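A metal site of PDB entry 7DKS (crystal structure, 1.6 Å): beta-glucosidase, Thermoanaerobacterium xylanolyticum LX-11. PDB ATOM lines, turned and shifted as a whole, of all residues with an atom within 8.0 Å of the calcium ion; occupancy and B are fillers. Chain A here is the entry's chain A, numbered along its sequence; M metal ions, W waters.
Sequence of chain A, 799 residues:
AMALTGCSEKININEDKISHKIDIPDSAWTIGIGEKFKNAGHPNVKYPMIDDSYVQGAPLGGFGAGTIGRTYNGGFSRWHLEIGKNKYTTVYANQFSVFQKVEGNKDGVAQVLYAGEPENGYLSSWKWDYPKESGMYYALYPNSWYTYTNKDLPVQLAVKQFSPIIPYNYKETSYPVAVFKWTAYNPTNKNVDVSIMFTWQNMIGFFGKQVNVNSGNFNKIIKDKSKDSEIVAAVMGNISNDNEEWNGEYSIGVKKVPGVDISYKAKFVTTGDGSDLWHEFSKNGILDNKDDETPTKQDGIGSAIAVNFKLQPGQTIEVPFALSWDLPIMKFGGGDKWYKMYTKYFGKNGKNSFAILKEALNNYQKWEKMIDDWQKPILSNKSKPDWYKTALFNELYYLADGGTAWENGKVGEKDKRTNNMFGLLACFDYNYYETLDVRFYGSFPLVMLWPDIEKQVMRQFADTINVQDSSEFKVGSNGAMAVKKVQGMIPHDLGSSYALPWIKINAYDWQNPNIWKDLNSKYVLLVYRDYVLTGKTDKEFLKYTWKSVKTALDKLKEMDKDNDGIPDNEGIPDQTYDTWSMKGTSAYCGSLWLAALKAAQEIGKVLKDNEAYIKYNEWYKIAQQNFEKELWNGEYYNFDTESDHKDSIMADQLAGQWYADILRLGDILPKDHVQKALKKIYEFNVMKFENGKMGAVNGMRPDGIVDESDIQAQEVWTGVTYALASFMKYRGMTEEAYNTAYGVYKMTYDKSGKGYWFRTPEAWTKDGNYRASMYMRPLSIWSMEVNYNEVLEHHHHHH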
ATOM      1  N   LYS A 557      17.042 -17.922  24.277  1.00  0.00           N
ATOM      2  CA  LYS A 557      17.520 -18.304  22.946  1.00  0.00           C
ATOM      3  C   LYS A 557      17.262 -17.211  21.901  1.00  0.00           C
ATOM      4  O   LYS A 557      18.084 -17.030  21.010  1.00  0.00           O
ATOM      5  CB  LYS A 557      16.864 -19.624  22.523  1.00  0.00           C
ATOM      6  CG  LYS A 557      17.315 -20.204  21.185  1.00  0.00           C
ATOM      7  CD  LYS A 557      18.823 -20.375  21.119  1.00  0.00           C
ATOM      8  CE  LYS A 557      19.223 -21.565  20.266  1.00  0.00           C
ATOM      9  NZ  LYS A 557      18.779 -21.384  18.859  1.00  0.00           N
ATOM     10  N   MET A 559      17.645 -14.115  22.306  1.00  0.00           N
ATOM     11  CA  MET A 559      18.690 -13.099  22.458  1.00  0.00           C
ATOM     12  C   MET A 559      20.014 -13.476  21.780  1.00  0.00           C
ATOM     13  O   MET A 559      20.987 -12.724  21.855  1.00  0.00           O
ATOM     14  CB  MET A 559      18.902 -12.810  23.936  1.00  0.00           C
ATOM     15  CG  MET A 559      17.660 -12.222  24.579  1.00  0.00           C
ATOM     16  SD  MET A 559      17.822 -12.113  26.370  1.00  0.00           S
ATOM     17  CE  MET A 559      16.293 -11.260  26.757  1.00  0.00           C
ATOM     18  N   ASP A 560      20.060 -14.628  21.117  1.00  0.00           N
ATOM     19  CA  ASP A 560      21.183 -14.962  20.247  1.00  0.00           C
ATOM     20  C   ASP A 560      21.084 -14.118  18.968  1.00  0.00           C
ATOM     21  O   ASP A 560      20.293 -14.435  18.103  1.00  0.00           O
ATOM     22  CB  ASP A 560      21.160 -16.452  19.911  1.00  0.00           C
ATOM     23  CG  ASP A 560      22.264 -16.871  18.955  1.00  0.00           C
ATOM     24  OD1 ASP A 560      23.227 -16.108  18.731  1.00  0.00           O
ATOM     25  OD2 ASP A 560      22.176 -17.988  18.424  1.00  0.00           O
ATOM     26  N   LYS A 561      21.910 -13.076  18.869  1.00  0.00           N
ATOM     27  CA  LYS A 561      21.914 -12.171  17.714  1.00  0.00           C
ATOM     28  C   LYS A 561      22.601 -12.724  16.466  1.00  0.00           C
ATOM     29  O   LYS A 561      22.142 -12.462  15.348  1.00  0.00           O
ATOM     30  CB  LYS A 561      22.600 -10.846  18.080  1.00  0.00           C
ATOM     31  CG  LYS A 561      21.866  -9.992  19.082  1.00  0.00           C
ATOM     32  CD  LYS A 561      22.741  -8.822  19.510  1.00  0.00           C
ATOM     33  CE  LYS A 561      21.926  -7.693  20.142  1.00  0.00           C
ATOM     34  NZ  LYS A 561      22.827  -6.578  20.568  1.00  0.00           N
ATOM     35  N   ASP A 562      23.698 -13.449  16.636  1.00  0.00           N
ATOM     36  CA  ASP A 562      24.560 -13.864  15.510  1.00  0.00           C
ATOM     37  C   ASP A 562      24.457 -15.360  15.141  1.00  0.00           C
ATOM     38  O   ASP A 562      25.311 -15.885  14.421  1.00  0.00           O
ATOM     39  CB  ASP A 562      26.017 -13.480  15.805  1.00  0.00           C
ATOM     40  CG  ASP A 562      26.626 -14.309  16.931  1.00  0.00           C
ATOM     41  OD1 ASP A 562      25.852 -14.927  17.697  1.00  0.00           O
ATOM     42  OD2 ASP A 562      27.859 -14.332  17.064  1.00  0.00           O
ATOM     43  N   ASN A 563      23.437 -16.030  15.665  1.00  0.00           N
ATOM     44  CA  ASN A 563      23.170 -17.445  15.378  1.00  0.00           C
ATOM     45  C   ASN A 563      24.296 -18.453  15.724  1.00  0.00           C
ATOM     46  O   ASN A 563      24.425 -19.501  15.087  1.00  0.00           O
ATOM     47  CB  ASN A 563      22.717 -17.610  13.916  1.00  0.00           C
ATOM     48  CG  ASN A 563      21.926 -18.891  13.684  1.00  0.00           C
ATOM     49  OD1 ASN A 563      21.327 -19.454  14.604  1.00  0.00           O
ATOM     50  ND2 ASN A 563      21.913 -19.363  12.433  1.00  0.00           N
ATOM     51  N   ASP A 564      25.099 -18.166  16.754  1.00  0.00           N
ATOM     52  CA  ASP A 564      26.058 -19.155  17.272  1.00  0.00           C
ATOM     53  C   ASP A 564      25.437 -20.092  18.353  1.00  0.00           C
ATOM     54  O   ASP A 564      26.148 -20.908  18.941  1.00  0.00           O
ATOM     55  CB  ASP A 564      27.345 -18.475  17.773  1.00  0.00           C
ATOM     56  CG  ASP A 564      27.165 -17.750  19.115  1.00  0.00           C
ATOM     57  OD1 ASP A 564      26.020 -17.592  19.559  1.00  0.00           O
ATOM     58  OD2 ASP A 564      28.164 -17.300  19.696  1.00  0.00           O
ATOM     59  N   GLY A 565      24.133 -19.940  18.607  1.00  0.00           N
ATOM     60  CA  GLY A 565      23.391 -20.783  19.546  1.00  0.00           C
ATOM     61  C   GLY A 565      23.511 -20.339  21.006  1.00  0.00           C
ATOM     62  O   GLY A 565      23.098 -21.083  21.897  1.00  0.00           O
ATOM     63  N   ILE A 566      24.063 -19.153  21.232  1.00  0.00           N
ATOM     64  CA  ILE A 566      24.321 -18.629  22.592  1.00  0.00           C
ATOM     65  C   ILE A 566      23.753 -17.208  22.667  1.00  0.00           C
ATOM     66  O   ILE A 566      23.957 -16.405  21.746  1.00  0.00           O
ATOM     67  CB  ILE A 566      25.842 -18.583  22.900  1.00  0.00           C
ATOM     68  CG1 ILE A 566      26.484 -19.957  22.658  1.00  0.00           C
ATOM     69  CG2 ILE A 566      26.093 -18.167  24.346  1.00  0.00           C
ATOM     70  CD1 ILE A 566      27.990 -19.966  22.750  1.00  0.00           C
ATOM     71  N   PRO A 567      23.051 -16.859  23.764  1.00  0.00           N
ATOM     72  CA  PRO A 567      22.627 -15.456  23.890  1.00  0.00           C
ATOM     73  C   PRO A 567      23.793 -14.470  23.884  1.00  0.00           C
ATOM     74  O   PRO A 567      24.874 -14.793  24.381  1.00  0.00           O
ATOM     75  CB  PRO A 567      21.886 -15.411  25.237  1.00  0.00           C
ATOM     76  CG  PRO A 567      22.370 -16.600  25.981  1.00  0.00           C
ATOM     77  CD  PRO A 567      22.664 -17.647  24.950  1.00  0.00           C
ATOM     78  N   ASP A 568      23.588 -13.303  23.269  1.00  0.00           N
ATOM     79  CA  ASP A 568      24.625 -12.271  23.167  1.00  0.00           C
ATOM     80  C   ASP A 568      24.483 -11.255  24.280  1.00  0.00           C
ATOM     81  O   ASP A 568      23.424 -10.642  24.388  1.00  0.00           O
ATOM     82  CB  ASP A 568      24.523 -11.513  21.837  1.00  0.00           C
ATOM     83  CG  ASP A 568      25.077 -12.301  20.672  1.00  0.00           C
ATOM     84  OD1 ASP A 568      24.433 -13.302  20.274  1.00  0.00           O
ATOM     85  OD2 ASP A 568      26.174 -11.951  20.195  1.00  0.00           O
ATOM     86  N   ASN A 569      25.541 -11.035  25.057  1.00  0.00           N
ATOM     87  CA  ASN A 569      25.588  -9.902  25.963  1.00  0.00           C
ATOM     88  C   ASN A 569      25.644  -8.638  25.093  1.00  0.00           C
ATOM     89  O   ASN A 569      26.262  -8.647  24.022  1.00  0.00           O
ATOM     90  CB  ASN A 569      26.778  -9.996  26.908  1.00  0.00           C
ATOM     91  CG  ASN A 569      26.668 -11.158  27.901  1.00  0.00           C
ATOM     92  OD1 ASN A 569      27.227 -12.233  27.676  1.00  0.00           O
ATOM     93  ND2 ASN A 569      25.947 -10.939  28.992  1.00  0.00           N
ATOM     94  N   GLY A 584      28.895  -9.861  23.409  1.00  0.00           N
ATOM     95  CA  GLY A 584      29.010 -11.077  22.608  1.00  0.00           C
ATOM     96  C   GLY A 584      28.784 -12.313  23.450  1.00  0.00           C
ATOM     97  O   GLY A 584      27.861 -12.332  24.284  1.00  0.00           O
ATOM     98  N   THR A 585      29.588 -13.344  23.228  1.00  0.00           N
ATOM     99  CA  THR A 585      29.560 -14.539  24.060  1.00  0.00           C
ATOM    100  C   THR A 585      30.482 -14.306  25.241  1.00  0.00           C
ATOM    101  O   THR A 585      31.675 -14.046  25.054  1.00  0.00           O
ATOM    102  CB  THR A 585      29.994 -15.781  23.273  1.00  0.00           C
ATOM    103  OG1 THR A 585      29.079 -16.001  22.191  1.00  0.00           O
ATOM    104  CG2 THR A 585      29.976 -17.013  24.164  1.00  0.00           C
ATOM    105  N   TRP A 593      24.476 -20.790  30.472  1.00  0.00           N
ATOM    106  CA  TRP A 593      23.588 -21.245  29.413  1.00  0.00           C
ATOM    107  C   TRP A 593      23.828 -22.707  29.064  1.00  0.00           C
ATOM    108  O   TRP A 593      22.895 -23.491  28.992  1.00  0.00           O
ATOM    109  CB  TRP A 593      23.779 -20.345  28.182  1.00  0.00           C
ATOM    110  CG  TRP A 593      23.094 -20.728  26.894  1.00  0.00           C
ATOM    111  CD1 TRP A 593      23.710 -21.034  25.721  1.00  0.00           C
ATOM    112  CD2 TRP A 593      21.685 -20.767  26.636  1.00  0.00           C
ATOM    113  NE1 TRP A 593      22.768 -21.272  24.741  1.00  0.00           N
ATOM    114  CE2 TRP A 593      21.521 -21.121  25.280  1.00  0.00           C
ATOM    115  CE3 TRP A 593      20.538 -20.548  27.417  1.00  0.00           C
ATOM    116  CZ2 TRP A 593      20.257 -21.267  24.681  1.00  0.00           C
ATOM    117  CZ3 TRP A 593      19.284 -20.694  26.829  1.00  0.00           C
ATOM    118  CH2 TRP A 593      19.155 -21.050  25.468  1.00  0.00           C
ATOM    119  N   ASN A 626      30.545 -23.995  19.880  1.00  0.00           N
ATOM    120  CA  ASN A 626      30.857 -22.606  19.616  1.00  0.00           C
ATOM    121  C   ASN A 626      31.466 -21.861  20.817  1.00  0.00           C
ATOM    122  O   ASN A 626      32.318 -21.010  20.624  1.00  0.00           O
ATOM    123  CB  ASN A 626      29.631 -21.882  19.065  1.00  0.00           C
ATOM    124  CG  ASN A 626      29.282 -22.342  17.652  1.00  0.00           C
ATOM    125  OD1 ASN A 626      30.175 -22.723  16.901  1.00  0.00           O
ATOM    126  ND2 ASN A 626      28.026 -22.295  17.299  1.00  0.00           N
ATOM    127  N   GLU A 630      35.018 -20.089  20.426  1.00  0.00           N
ATOM    128  CA  GLU A 630      35.099 -18.651  20.605  1.00  0.00           C
ATOM    129  C   GLU A 630      35.994 -18.204  21.755  1.00  0.00           C
ATOM    130  O   GLU A 630      36.609 -17.145  21.666  1.00  0.00           O
ATOM    131  CB  GLU A 630      33.702 -18.065  20.822  1.00  0.00           C
ATOM    132  CG  GLU A 630      32.839 -18.082  19.570  1.00  0.00           C
ATOM    133  CD  GLU A 630      31.368 -17.941  19.883  1.00  0.00           C
ATOM    134  OE1 GLU A 630      31.025 -17.493  21.001  1.00  0.00           O
ATOM    135  OE2 GLU A 630      30.546 -18.294  18.999  1.00  0.00           O
ATOM    136  N   THR A 641      33.772 -12.250  23.869  1.00  0.00           N
ATOM    137  CA  THR A 641      34.272 -12.180  22.471  1.00  0.00           C
ATOM    138  C   THR A 641      34.416 -10.770  21.889  1.00  0.00           C
ATOM    139  O   THR A 641      35.097 -10.619  20.871  1.00  0.00           O
ATOM    140  CB  THR A 641      33.367 -12.996  21.537  1.00  0.00           C
ATOM    141  OG1 THR A 641      32.016 -12.535  21.649  1.00  0.00           O
ATOM    142  CG2 THR A 641      33.442 -14.470  21.870  1.00  0.00           C
ATOM    143  N   GLU A 642      33.812  -9.756  22.505  1.00  0.00           N
ATOM    144  CA  GLU A 642      33.773  -8.401  21.893  1.00  0.00           C
ATOM    145  C   GLU A 642      34.186  -7.188  22.746  1.00  0.00           C
ATOM    146  O   GLU A 642      34.295  -6.090  22.200  1.00  0.00           O
ATOM    147  CB  GLU A 642      32.388  -8.152  21.313  1.00  0.00           C
ATOM    148  CG  GLU A 642      31.993  -9.128  20.223  1.00  0.00           C
ATOM    149  CD  GLU A 642      30.659  -8.786  19.583  1.00  0.00           C
ATOM    150  OE1 GLU A 642      30.393  -7.577  19.389  1.00  0.00           O
ATOM    151  OE2 GLU A 642      29.876  -9.698  19.282  1.00  0.00           O
HETATM  152 CA    CA M   1      25.191 -15.418  19.982  1.00  0.00          CA
HETATM  153  O   HOH W   1      26.554 -15.071  22.003  1.00  0.00           O
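Water W1 lies within hydrogen-bond range of OG1 of Thr 585 (2.7 Å) and O of Pro 567 (2.9 Å).
OD2 of Asp 564 sits at hydrogen-bond distance from OG1 of Thr 585, 3.0 Å away. N of Asp 568 lies within hydrogen-bond range of O of Met 559. The backbone carbonyl oxygen (O) of Asp 564 is in hydrogen-bond range of the side-chain amide nitrogen (ND2) of Asn 626. OD1 of Asp 560 lies close to N of Asn 563 (3.1 Å). The side-chain carboxylate (OD2) of Asp 564 sits close to the side-chain carboxylate (OE2) of Glu 630 (2.7 Å). OD2 of Asp 560 lies within hydrogen-bond range of N of Gly 565 (2.8 Å). The backbone NH of Lys 561 sits close to the side-chain carboxylate of Asp 568 (2.9 Å).
Within 4 Å of the calcium ion: Asp 560, Asp 562, Asp 564, Ile 566 and Asp 568. The nearest printed residue that does not touch the calcium ion is Lys 561 (4.2 Å).
The calcium ion is bound by the side-chain carboxylate of Asp 568 (2.3 Å), the side-chain carboxylate of Asp 564 (2.4 Å), the backbone carbonyl oxygen of Ile 566 (2.4 Å), the side-chain carboxylate of Asp 562 (2.4 Å), the side-chain carboxylate of Asp 560 (2.4 Å) and water W1 (2.5 Å).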
